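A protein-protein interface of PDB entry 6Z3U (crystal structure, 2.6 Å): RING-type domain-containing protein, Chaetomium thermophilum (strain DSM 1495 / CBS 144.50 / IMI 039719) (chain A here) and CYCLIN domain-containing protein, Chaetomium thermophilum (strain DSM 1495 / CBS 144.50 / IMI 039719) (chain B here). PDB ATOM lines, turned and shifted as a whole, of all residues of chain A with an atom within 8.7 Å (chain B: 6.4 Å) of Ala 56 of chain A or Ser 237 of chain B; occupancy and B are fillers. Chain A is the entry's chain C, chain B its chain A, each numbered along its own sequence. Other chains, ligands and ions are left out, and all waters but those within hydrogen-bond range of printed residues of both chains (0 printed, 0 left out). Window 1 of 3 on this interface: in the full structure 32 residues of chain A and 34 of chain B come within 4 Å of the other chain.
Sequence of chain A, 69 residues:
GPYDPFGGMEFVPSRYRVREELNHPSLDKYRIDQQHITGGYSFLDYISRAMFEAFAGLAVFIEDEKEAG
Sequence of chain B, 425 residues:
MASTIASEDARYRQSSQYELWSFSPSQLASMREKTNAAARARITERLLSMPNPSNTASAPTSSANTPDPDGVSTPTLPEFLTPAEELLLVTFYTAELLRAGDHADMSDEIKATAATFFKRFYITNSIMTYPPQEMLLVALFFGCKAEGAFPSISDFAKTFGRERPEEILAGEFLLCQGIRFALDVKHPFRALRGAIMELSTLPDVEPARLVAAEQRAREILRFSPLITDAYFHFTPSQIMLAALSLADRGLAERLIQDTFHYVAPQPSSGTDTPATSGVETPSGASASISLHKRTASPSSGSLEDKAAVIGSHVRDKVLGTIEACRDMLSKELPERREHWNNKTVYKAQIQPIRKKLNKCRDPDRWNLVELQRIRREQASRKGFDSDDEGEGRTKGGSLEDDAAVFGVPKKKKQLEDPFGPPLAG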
ATOM      1  N   PHE A  11     -16.704  28.620  16.007  1.00  0.00           N
ATOM      2  CA  PHE A  11     -16.778  27.312  15.373  1.00  0.00           C
ATOM      3  C   PHE A  11     -16.562  27.469  13.873  1.00  0.00           C
ATOM      4  O   PHE A  11     -17.348  28.140  13.195  1.00  0.00           O
ATOM      5  CB  PHE A  11     -18.123  26.644  15.648  1.00  0.00           C
ATOM      6  CG  PHE A  11     -18.370  25.424  14.810  1.00  0.00           C
ATOM      7  CD1 PHE A  11     -17.678  24.249  15.052  1.00  0.00           C
ATOM      8  CD2 PHE A  11     -19.284  25.455  13.771  1.00  0.00           C
ATOM      9  CE1 PHE A  11     -17.899  23.125  14.279  1.00  0.00           C
ATOM     10  CE2 PHE A  11     -19.510  24.337  12.994  1.00  0.00           C
ATOM     11  CZ  PHE A  11     -18.816  23.169  13.248  1.00  0.00           C
ATOM     12  N   PRO A  13     -16.138  24.964  10.686  1.00  0.00           N
ATOM     13  CA  PRO A  13     -16.125  23.564  10.249  1.00  0.00           C
ATOM     14  C   PRO A  13     -14.898  23.250   9.407  1.00  0.00           C
ATOM     15  O   PRO A  13     -14.353  24.111   8.713  1.00  0.00           O
ATOM     16  CB  PRO A  13     -17.418  23.430   9.435  1.00  0.00           C
ATOM     17  CG  PRO A  13     -17.756  24.819   9.022  1.00  0.00           C
ATOM     18  CD  PRO A  13     -17.297  25.696  10.142  1.00  0.00           C
ATOM     19  N   ARG A  15     -14.446  19.880   7.511  1.00  0.00           N
ATOM     20  CA  ARG A  15     -14.669  19.017   6.362  1.00  0.00           C
ATOM     21  C   ARG A  15     -15.827  19.472   5.484  1.00  0.00           C
ATOM     22  O   ARG A  15     -16.099  18.833   4.464  1.00  0.00           O
ATOM     23  CB  ARG A  15     -14.934  17.582   6.829  1.00  0.00           C
ATOM     24  CG  ARG A  15     -13.854  17.006   7.724  1.00  0.00           C
ATOM     25  CD  ARG A  15     -13.859  15.489   7.700  1.00  0.00           C
ATOM     26  NE  ARG A  15     -12.937  14.935   8.687  1.00  0.00           N
ATOM     27  CZ  ARG A  15     -13.226  14.784   9.977  1.00  0.00           C
ATOM     28  NH1 ARG A  15     -14.412  15.147  10.449  1.00  0.00           N
ATOM     29  NH2 ARG A  15     -12.323  14.273  10.802  1.00  0.00           N
ATOM     30  N   TYR A  16     -16.514  20.551   5.851  1.00  0.00           N
ATOM     31  CA  TYR A  16     -17.650  21.014   5.069  1.00  0.00           C
ATOM     32  C   TYR A  16     -17.742  22.528   5.148  1.00  0.00           C
ATOM     33  O   TYR A  16     -17.124  23.169   6.002  1.00  0.00           O
ATOM     34  CB  TYR A  16     -18.959  20.372   5.548  1.00  0.00           C
ATOM     35  CG  TYR A  16     -19.466  20.901   6.871  1.00  0.00           C
ATOM     36  CD1 TYR A  16     -19.055  20.337   8.072  1.00  0.00           C
ATOM     37  CD2 TYR A  16     -20.371  21.955   6.920  1.00  0.00           C
ATOM     38  CE1 TYR A  16     -19.520  20.813   9.281  1.00  0.00           C
ATOM     39  CE2 TYR A  16     -20.842  22.436   8.125  1.00  0.00           C
ATOM     40  CZ  TYR A  16     -20.415  21.861   9.303  1.00  0.00           C
ATOM     41  OH  TYR A  16     -20.880  22.339  10.505  1.00  0.00           O
ATOM     42  N   ARG A  49     -27.785  23.887  10.449  1.00  0.00           N
ATOM     43  CA  ARG A  49     -28.011  22.864  11.464  1.00  0.00           C
ATOM     44  C   ARG A  49     -27.892  21.467  10.870  1.00  0.00           C
ATOM     45  O   ARG A  49     -27.307  20.571  11.490  1.00  0.00           O
ATOM     46  CB  ARG A  49     -29.387  23.082  12.096  1.00  0.00           C
ATOM     47  CG  ARG A  49     -29.761  22.132  13.224  1.00  0.00           C
ATOM     48  CD  ARG A  49     -30.867  22.746  14.078  1.00  0.00           C
ATOM     49  NE  ARG A  49     -31.737  21.755  14.705  1.00  0.00           N
ATOM     50  CZ  ARG A  49     -31.415  21.044  15.781  1.00  0.00           C
ATOM     51  NH1 ARG A  49     -32.280  20.175  16.283  1.00  0.00           N
ATOM     52  NH2 ARG A  49     -30.226  21.188  16.351  1.00  0.00           N
ATOM     53  N   ALA A  50     -28.432  21.266   9.667  1.00  0.00           N
ATOM     54  CA  ALA A  50     -28.361  19.957   9.028  1.00  0.00           C
ATOM     55  C   ALA A  50     -26.927  19.603   8.647  1.00  0.00           C
ATOM     56  O   ALA A  50     -26.461  18.490   8.910  1.00  0.00           O
ATOM     57  CB  ALA A  50     -29.265  19.928   7.794  1.00  0.00           C
ATOM     58  N   MET A  51     -26.212  20.546   8.029  1.00  0.00           N
ATOM     59  CA  MET A  51     -24.852  20.268   7.573  1.00  0.00           C
ATOM     60  C   MET A  51     -23.934  19.912   8.736  1.00  0.00           C
ATOM     61  O   MET A  51     -23.086  19.020   8.615  1.00  0.00           O
ATOM     62  CB  MET A  51     -24.308  21.476   6.809  1.00  0.00           C
ATOM     63  CG  MET A  51     -25.000  21.724   5.479  1.00  0.00           C
ATOM     64  SD  MET A  51     -24.644  20.451   4.255  1.00  0.00           S
ATOM     65  CE  MET A  51     -23.046  20.996   3.656  1.00  0.00           C
ATOM     66  N   PHE A  52     -24.085  20.595   9.872  1.00  0.00           N
ATOM     67  CA  PHE A  52     -23.274  20.264  11.039  1.00  0.00           C
ATOM     68  C   PHE A  52     -23.527  18.831  11.487  1.00  0.00           C
ATOM     69  O   PHE A  52     -22.590  18.039  11.640  1.00  0.00           O
ATOM     70  CB  PHE A  52     -23.573  21.241  12.176  1.00  0.00           C
ATOM     71  CG  PHE A  52     -22.855  20.921  13.455  1.00  0.00           C
ATOM     72  CD1 PHE A  52     -21.520  21.250  13.615  1.00  0.00           C
ATOM     73  CD2 PHE A  52     -23.517  20.296  14.498  1.00  0.00           C
ATOM     74  CE1 PHE A  52     -20.857  20.958  14.792  1.00  0.00           C
ATOM     75  CE2 PHE A  52     -22.860  20.002  15.677  1.00  0.00           C
ATOM     76  CZ  PHE A  52     -21.527  20.334  15.825  1.00  0.00           C
ATOM     77  N   GLU A  53     -24.795  18.477  11.693  1.00  0.00           N
ATOM     78  CA  GLU A  53     -25.119  17.139  12.171  1.00  0.00           C
ATOM     79  C   GLU A  53     -24.738  16.074  11.154  1.00  0.00           C
ATOM     80  O   GLU A  53     -24.471  14.927  11.530  1.00  0.00           O
ATOM     81  CB  GLU A  53     -26.607  17.063  12.512  1.00  0.00           C
ATOM     82  CG  GLU A  53     -27.005  17.992  13.659  1.00  0.00           C
ATOM     83  CD  GLU A  53     -28.501  18.036  13.901  1.00  0.00           C
ATOM     84  OE1 GLU A  53     -29.235  17.257  13.257  1.00  0.00           O
ATOM     85  OE2 GLU A  53     -28.943  18.859  14.731  1.00  0.00           O
ATOM     86  N   ALA A  54     -24.706  16.429   9.865  1.00  0.00           N
ATOM     87  CA  ALA A  54     -24.325  15.463   8.840  1.00  0.00           C
ATOM     88  C   ALA A  54     -22.840  15.127   8.900  1.00  0.00           C
ATOM     89  O   ALA A  54     -22.437  14.035   8.484  1.00  0.00           O
ATOM     90  CB  ALA A  54     -24.686  15.997   7.453  1.00  0.00           C
ATOM     91  N   PHE A  55     -22.014  16.046   9.402  1.00  0.00           N
ATOM     92  CA  PHE A  55     -20.579  15.830   9.494  1.00  0.00           C
ATOM     93  C   PHE A  55     -20.056  15.783  10.922  1.00  0.00           C
ATOM     94  O   PHE A  55     -18.901  15.391  11.124  1.00  0.00           O
ATOM     95  CB  PHE A  55     -19.823  16.932   8.733  1.00  0.00           C
ATOM     96  CG  PHE A  55     -19.966  16.848   7.240  1.00  0.00           C
ATOM     97  CD1 PHE A  55     -21.043  17.436   6.597  1.00  0.00           C
ATOM     98  CD2 PHE A  55     -19.017  16.187   6.477  1.00  0.00           C
ATOM     99  CE1 PHE A  55     -21.175  17.361   5.222  1.00  0.00           C
ATOM    100  CE2 PHE A  55     -19.142  16.108   5.102  1.00  0.00           C
ATOM    101  CZ  PHE A  55     -20.223  16.696   4.473  1.00  0.00           C
ATOM    102  N   ALA A  56     -20.863  16.155  11.913  1.00  0.00           N
ATOM    103  CA  ALA A  56     -20.395  16.176  13.293  1.00  0.00           C
ATOM    104  C   ALA A  56     -20.053  14.768  13.755  1.00  0.00           C
ATOM    105  O   ALA A  56     -20.929  13.902  13.839  1.00  0.00           O
ATOM    106  CB  ALA A  56     -21.459  16.792  14.197  1.00  0.00           C
ATOM    107  N   GLY A  57     -18.778  14.545  14.061  1.00  0.00           N
ATOM    108  CA  GLY A  57     -18.330  13.245  14.515  1.00  0.00           C
ATOM    109  C   GLY A  57     -18.170  12.220  13.418  1.00  0.00           C
ATOM    110  O   GLY A  57     -18.336  11.022  13.668  1.00  0.00           O
ATOM    111  N   LEU A  58     -17.839  12.655  12.200  1.00  0.00           N
ATOM    112  CA  LEU A  58     -17.654  11.706  11.109  1.00  0.00           C
ATOM    113  C   LEU A  58     -16.439  10.821  11.359  1.00  0.00           C
ATOM    114  O   LEU A  58     -16.446   9.634  11.013  1.00  0.00           O
ATOM    115  CB  LEU A  58     -17.512  12.451   9.783  1.00  0.00           C
ATOM    116  CG  LEU A  58     -18.135  11.778   8.555  1.00  0.00           C
ATOM    117  CD1 LEU A  58     -17.711  12.495   7.277  1.00  0.00           C
ATOM    118  CD2 LEU A  58     -17.779  10.301   8.488  1.00  0.00           C
ATOM    119  N   ALA A  59     -15.389  11.379  11.963  1.00  0.00           N
ATOM    120  CA  ALA A  59     -14.180  10.637  12.292  1.00  0.00           C
ATOM    121  C   ALA A  59     -14.094  10.335  13.784  1.00  0.00           C
ATOM    122  O   ALA A  59     -13.002  10.158  14.329  1.00  0.00           O
ATOM    123  CB  ALA A  59     -12.938  11.401  11.837  1.00  0.00           C
ATOM    124  N   VAL A  60     -15.242  10.282  14.456  1.00  0.00           N
ATOM    125  CA  VAL A  60     -15.313   9.903  15.863  1.00  0.00           C
ATOM    126  C   VAL A  60     -15.569   8.400  15.894  1.00  0.00           C
ATOM    127  O   VAL A  60     -16.683   7.940  15.639  1.00  0.00           O
ATOM    128  CB  VAL A  60     -16.392  10.685  16.610  1.00  0.00           C
ATOM    129  CG1 VAL A  60     -16.682  10.043  17.960  1.00  0.00           C
ATOM    130  CG2 VAL A  60     -15.958  12.128  16.800  1.00  0.00           C
ATOM    131  N   GLU B   8     -15.779  19.920  14.178  1.00  0.00           N
ATOM    132  CA  GLU B   8     -17.117  19.384  14.406  1.00  0.00           C
ATOM    133  C   GLU B   8     -17.067  18.068  15.174  1.00  0.00           C
ATOM    134  O   GLU B   8     -18.032  17.718  15.862  1.00  0.00           O
ATOM    135  CB  GLU B   8     -17.855  19.188  13.080  1.00  0.00           C
ATOM    136  CG  GLU B   8     -17.177  18.244  12.099  1.00  0.00           C
ATOM    137  CD  GLU B   8     -16.357  18.970  11.056  1.00  0.00           C
ATOM    138  OE1 GLU B   8     -15.579  19.872  11.427  1.00  0.00           O
ATOM    139  OE2 GLU B   8     -16.494  18.636   9.861  1.00  0.00           O
ATOM    140  N   ASP B   9     -15.961  17.325  15.064  1.00  0.00           N
ATOM    141  CA  ASP B   9     -15.812  16.105  15.852  1.00  0.00           C
ATOM    142  C   ASP B   9     -15.533  16.427  17.315  1.00  0.00           C
ATOM    143  O   ASP B   9     -16.049  15.754  18.214  1.00  0.00           O
ATOM    144  CB  ASP B   9     -14.696  15.232  15.275  1.00  0.00           C
ATOM    145  CG  ASP B   9     -15.037  14.675  13.902  1.00  0.00           C
ATOM    146  OD1 ASP B   9     -16.190  14.846  13.452  1.00  0.00           O
ATOM    147  OD2 ASP B   9     -14.151  14.060  13.273  1.00  0.00           O
ATOM    148  N   TYR B  12     -18.714  17.329  19.041  1.00  0.00           N
ATOM    149  CA  TYR B  12     -19.581  16.180  19.273  1.00  0.00           C
ATOM    150  C   TYR B  12     -19.161  15.414  20.523  1.00  0.00           C
ATOM    151  O   TYR B  12     -20.014  14.977  21.305  1.00  0.00           O
ATOM    152  CB  TYR B  12     -19.575  15.250  18.059  1.00  0.00           C
ATOM    153  CG  TYR B  12     -20.462  14.038  18.242  1.00  0.00           C
ATOM    154  CD1 TYR B  12     -21.816  14.092  17.943  1.00  0.00           C
ATOM    155  CD2 TYR B  12     -19.947  12.845  18.734  1.00  0.00           C
ATOM    156  CE1 TYR B  12     -22.632  12.989  18.118  1.00  0.00           C
ATOM    157  CE2 TYR B  12     -20.755  11.737  18.913  1.00  0.00           C
ATOM    158  CZ  TYR B  12     -22.096  11.815  18.605  1.00  0.00           C
ATOM    159  OH  TYR B  12     -22.902  10.714  18.781  1.00  0.00           O
ATOM    160  N   PRO B 188     -30.134  11.197  13.358  1.00  0.00           N
ATOM    161  CA  PRO B 188     -29.582  11.415  12.009  1.00  0.00           C
ATOM    162  C   PRO B 188     -30.599  11.850  10.961  1.00  0.00           C
ATOM    163  O   PRO B 188     -30.229  11.929   9.784  1.00  0.00           O
ATOM    164  CB  PRO B 188     -29.024  10.026  11.663  1.00  0.00           C
ATOM    165  CG  PRO B 188     -29.655   9.045  12.666  1.00  0.00           C
ATOM    166  CD  PRO B 188     -30.628   9.820  13.501  1.00  0.00           C
ATOM    167  N   ALA B 191     -29.552  15.179   9.692  1.00  0.00           N
ATOM    168  CA  ALA B 191     -28.289  14.931   9.005  1.00  0.00           C
ATOM    169  C   ALA B 191     -28.513  14.387   7.600  1.00  0.00           C
ATOM    170  O   ALA B 191     -27.745  14.696   6.682  1.00  0.00           O
ATOM    171  CB  ALA B 191     -27.435  13.962   9.819  1.00  0.00           C
ATOM    172  N   PHE B 234     -21.991   4.257  17.029  1.00  0.00           N
ATOM    173  CA  PHE B 234     -21.779   5.089  15.856  1.00  0.00           C
ATOM    174  C   PHE B 234     -22.408   6.456  16.068  1.00  0.00           C
ATOM    175  O   PHE B 234     -23.344   6.619  16.855  1.00  0.00           O
ATOM    176  CB  PHE B 234     -22.356   4.428  14.598  1.00  0.00           C
ATOM    177  CG  PHE B 234     -21.833   3.043  14.353  1.00  0.00           C
ATOM    178  CD1 PHE B 234     -20.577   2.849  13.804  1.00  0.00           C
ATOM    179  CD2 PHE B 234     -22.597   1.934  14.675  1.00  0.00           C
ATOM    180  CE1 PHE B 234     -20.093   1.576  13.580  1.00  0.00           C
ATOM    181  CE2 PHE B 234     -22.119   0.658  14.451  1.00  0.00           C
ATOM    182  CZ  PHE B 234     -20.865   0.479  13.902  1.00  0.00           C
ATOM    183  N   THR B 235     -21.876   7.426  15.368  1.00  0.00           N
ATOM    184  CA  THR B 235     -22.280   8.821  15.393  1.00  0.00           C
ATOM    185  C   THR B 235     -23.436   9.053  14.425  1.00  0.00           C
ATOM    186  O   THR B 235     -23.550   8.357  13.412  1.00  0.00           O
ATOM    187  CB  THR B 235     -21.095   9.704  15.012  1.00  0.00           C
ATOM    188  OG1 THR B 235     -20.028   9.489  15.945  1.00  0.00           O
ATOM    189  CG2 THR B 235     -21.462  11.172  15.016  1.00  0.00           C
ATOM    190  N   PRO B 236     -24.327  10.012  14.709  1.00  0.00           N
ATOM    191  CA  PRO B 236     -25.417  10.289  13.757  1.00  0.00           C
ATOM    192  C   PRO B 236     -24.951  10.455  12.322  1.00  0.00           C
ATOM    193  O   PRO B 236     -25.633   9.989  11.401  1.00  0.00           O
ATOM    194  CB  PRO B 236     -26.034  11.576  14.317  1.00  0.00           C
ATOM    195  CG  PRO B 236     -25.840  11.444  15.789  1.00  0.00           C
ATOM    196  CD  PRO B 236     -24.504  10.757  15.970  1.00  0.00           C
ATOM    197  N   SER B 237     -23.807  11.106  12.099  1.00  0.00           N
ATOM    198  CA  SER B 237     -23.270  11.182  10.745  1.00  0.00           C
ATOM    199  C   SER B 237     -22.917   9.794  10.231  1.00  0.00           C
ATOM    200  O   SER B 237     -23.212   9.453   9.080  1.00  0.00           O
ATOM    201  CB  SER B 237     -22.040  12.087  10.709  1.00  0.00           C
ATOM    202  OG  SER B 237     -20.989  11.555  11.497  1.00  0.00           O
ATOM    203  N   GLN B 238     -22.290   8.976  11.077  1.00  0.00           N
ATOM    204  CA  GLN B 238     -21.927   7.623  10.671  1.00  0.00           C
ATOM    205  C   GLN B 238     -23.170   6.788  10.387  1.00  0.00           C
ATOM    206  O   GLN B 238     -23.250   6.102   9.362  1.00  0.00           O
ATOM    207  CB  GLN B 238     -21.068   6.976  11.758  1.00  0.00           C
ATOM    208  CG  GLN B 238     -19.718   7.651  11.950  1.00  0.00           C
ATOM    209  CD  GLN B 238     -18.991   7.166  13.189  1.00  0.00           C
ATOM    210  OE1 GLN B 238     -19.512   6.355  13.951  1.00  0.00           O
ATOM    211  NE2 GLN B 238     -17.780   7.667  13.396  1.00  0.00           N
ATOM    212  N   ILE B 239     -24.152   6.831  11.290  1.00  0.00           N
ATOM    213  CA  ILE B 239     -25.396   6.101  11.067  1.00  0.00           C
ATOM    214  C   ILE B 239     -26.111   6.632   9.832  1.00  0.00           C
ATOM    215  O   ILE B 239     -26.634   5.862   9.017  1.00  0.00           O
ATOM    216  CB  ILE B 239     -26.295   6.183  12.317  1.00  0.00           C
ATOM    217  CG1 ILE B 239     -25.613   5.507  13.508  1.00  0.00           C
ATOM    218  CG2 ILE B 239     -27.650   5.547  12.041  1.00  0.00           C
ATOM    219  CD1 ILE B 239     -26.327   5.723  14.822  1.00  0.00           C
ATOM    220  N   MET B 240     -26.153   7.958   9.678  1.00  0.00           N
ATOM    221  CA  MET B 240     -26.839   8.557   8.536  1.00  0.00           C
ATOM    222  C   MET B 240     -26.232   8.083   7.221  1.00  0.00           C
ATOM    223  O   MET B 240     -26.954   7.686   6.298  1.00  0.00           O
ATOM    224  CB  MET B 240     -26.787  10.082   8.642  1.00  0.00           C
ATOM    225  CG  MET B 240     -27.366  10.808   7.443  1.00  0.00           C
ATOM    226  SD  MET B 240     -26.136  11.110   6.164  1.00  0.00           S
ATOM    227  CE  MET B 240     -27.040  10.617   4.703  1.00  0.00           C
ATOM    228  N   LEU B 241     -24.903   8.127   7.112  1.00  0.00           N
ATOM    229  CA  LEU B 241     -24.248   7.648   5.899  1.00  0.00           C
ATOM    230  C   LEU B 241     -24.503   6.162   5.676  1.00  0.00           C
ATOM    231  O   LEU B 241     -24.610   5.715   4.529  1.00  0.00           O
ATOM    232  CB  LEU B 241     -22.745   7.926   5.969  1.00  0.00           C
ATOM    233  CG  LEU B 241     -22.319   9.395   5.888  1.00  0.00           C
ATOM    234  CD1 LEU B 241     -20.872   9.558   6.324  1.00  0.00           C
ATOM    235  CD2 LEU B 241     -22.513   9.940   4.481  1.00  0.00           C
ATOM    236  N   ALA B 242     -24.618   5.386   6.756  1.00  0.00           N
ATOM    237  CA  ALA B 242     -24.857   3.955   6.612  1.00  0.00           C
ATOM    238  C   ALA B 242     -26.240   3.681   6.037  1.00  0.00           C
ATOM    239  O   ALA B 242     -26.389   2.845   5.138  1.00  0.00           O
ATOM    240  CB  ALA B 242     -24.688   3.258   7.962  1.00  0.00           C
ATOM    241  N   ILE B 322     -18.247   3.016   8.618  1.00  0.00           N
ATOM    242  CA  ILE B 322     -19.579   3.020   8.021  1.00  0.00           C
ATOM    243  C   ILE B 322     -19.972   1.610   7.598  1.00  0.00           C
ATOM    244  O   ILE B 322     -21.129   1.199   7.752  1.00  0.00           O
ATOM    245  CB  ILE B 322     -19.639   3.997   6.833  1.00  0.00           C
ATOM    246  CG1 ILE B 322     -19.184   5.400   7.247  1.00  0.00           C
ATOM    247  CG2 ILE B 322     -21.051   4.047   6.261  1.00  0.00           C
ATOM    248  CD1 ILE B 322     -20.033   6.034   8.316  1.00  0.00           C
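NE2 of Gln 238 of chain B sits at hydrogen-bond distance from O of Gly 57 of chain A (3.4 Å). The backbone NH of Gly 57 of chain A is in hydrogen-bond range of the side-chain carboxylate of Asp 9 of chain B, 2.7 Å away. The side-chain carboxylate of Glu 8 of chain B sits at hydrogen-bond distance from the backbone NH of Arg 15 of chain A, 3.4 Å away. The backbone carbonyl oxygen of Val 60 of chain A lies within hydrogen-bond range of the side-chain amide nitrogen of Gln 238 of chain B. The guanidinium group of Arg 15 of chain A lies within salt-bridge range of the side-chain carboxylate of Asp 9 of chain B. The side-chain hydroxyl of Ser 237 of chain B sits at hydrogen-bond distance from the backbone carbonyl oxygen of Ala 56 of chain A (3.3 Å). The backbone NH (N) of Ala 59 of chain A is in hydrogen-bond range of the side-chain carboxylate (OD2) of Asp 9 of chain B (3.2 Å). The backbone carbonyl oxygen (O) of Gly 57 of chain A sits at hydrogen-bond distance from the side-chain hydroxyl (OG1) of Thr 235 of chain B (3.2 Å). The side-chain hydroxyl (OG) of Ser 237 of chain B lies close to the backbone NH (N) of Leu 58 of chain A, 3.4 Å away. OD1 of Asp 9 of chain B is in hydrogen-bond range of N of Leu 58 of chain A (3.0 Å). NE2 of Gln 238 of chain B sits at hydrogen-bond distance from O of Leu 58 of chain A (3.4 Å). OG of Ser 237 of chain B is in hydrogen-bond range of O of Gly 57 of chain A (3.5 Å).
The guanidinium group (NH2) of Arg 49 of chain A is in salt-bridge range of the side-chain carboxylate (OE2) of Glu 53 of chain A (3.1 Å). The backbone NH of Thr 235 of chain B sits at hydrogen-bond distance from the side-chain amide oxygen of Gln 238 of chain B (3.0 Å).
Among the printed residues, pairs that only touch across the chains: Ala 54 of chain A with Ser 237 of chain B (3.0 Å), Ala 56 of chain A with Thr 235 of chain B (3.0 Å), Ala 54 of chain A with Ala 191 of chain B (3.4 Å), Phe 55 of chain A with Glu 8 of chain B (3.5 Å), Glu 53 of chain A with Ala 191 of chain B (3.6 Å), Tyr 16 of chain A with Glu 8 of chain B (3.6 Å), Phe 55 of chain A with Asp 9 of chain B (3.6 Å), Val 60 of chain A with Asp 9 of chain B (3.7 Å), Val 60 of chain A with Thr 235 of chain B (3.7 Å), Gly 57 of chain A with Glu 8 of chain B (3.7 Å), Ala 56 of chain A with Glu 8 of chain B (3.8 Å), Phe 11 of chain A with Glu 8 of chain B (3.8 Å), Glu 53 of chain A with Ser 237 of chain B (3.8 Å), Leu 58 of chain A with Leu 241 of chain B (3.8 Å), Ala 56 of chain A with Asp 9 of chain B (3.9 Å), Phe 52 of chain A with Glu 8 of chain B (3.9 Å) and Pro 13 of chain A with Glu 8 of chain B (3.9 Å).
Ala 56 of chain A touches four residues of chain B. Ser 237 of chain B touches just these residues of chain A: Glu 53 (3.8 Å), Ala 54 (3.0 Å), Ala 56 (3.3 Å), Gly 57 (3.5 Å) and Leu 58 (3.4 Å). Of the printed residues of chain B, Glu 53 of chain A touches Ala 191 and Ser 237. Printed residues of chain A within 4 Å of Leu 241 of chain B: Leu 58. Phe 234 of chain B touches none of the printed residues of chain A. The nearest residue of chain B that does not touch Ala 56 of chain A is Tyr 12 of chain B (4.2 Å). The nearest printed residue of chain A that does not touch Ala 191 of chain B is Ala 50 of chain A (4.002 Å).
Of the 15 printed residues of chain B, 7 touch a printed residue of chain A. Printed residues of chain B that touch a printed residue of chain A: Glu 8, Asp 9, Ala 191, Thr 235, Ser 237, Gln 238 and Leu 241. Hydrophobic or aromatic side chains of chain B within 4 Å of the printed part of chain A: Ala 191 and Leu 241. Among the printed residues, Asp or Glu carboxylates within 4 Å of a Lys or Arg side-chain nitrogen of the other chain: Arg 15 of chain A with Asp 9 of chain B (3.0 Å).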
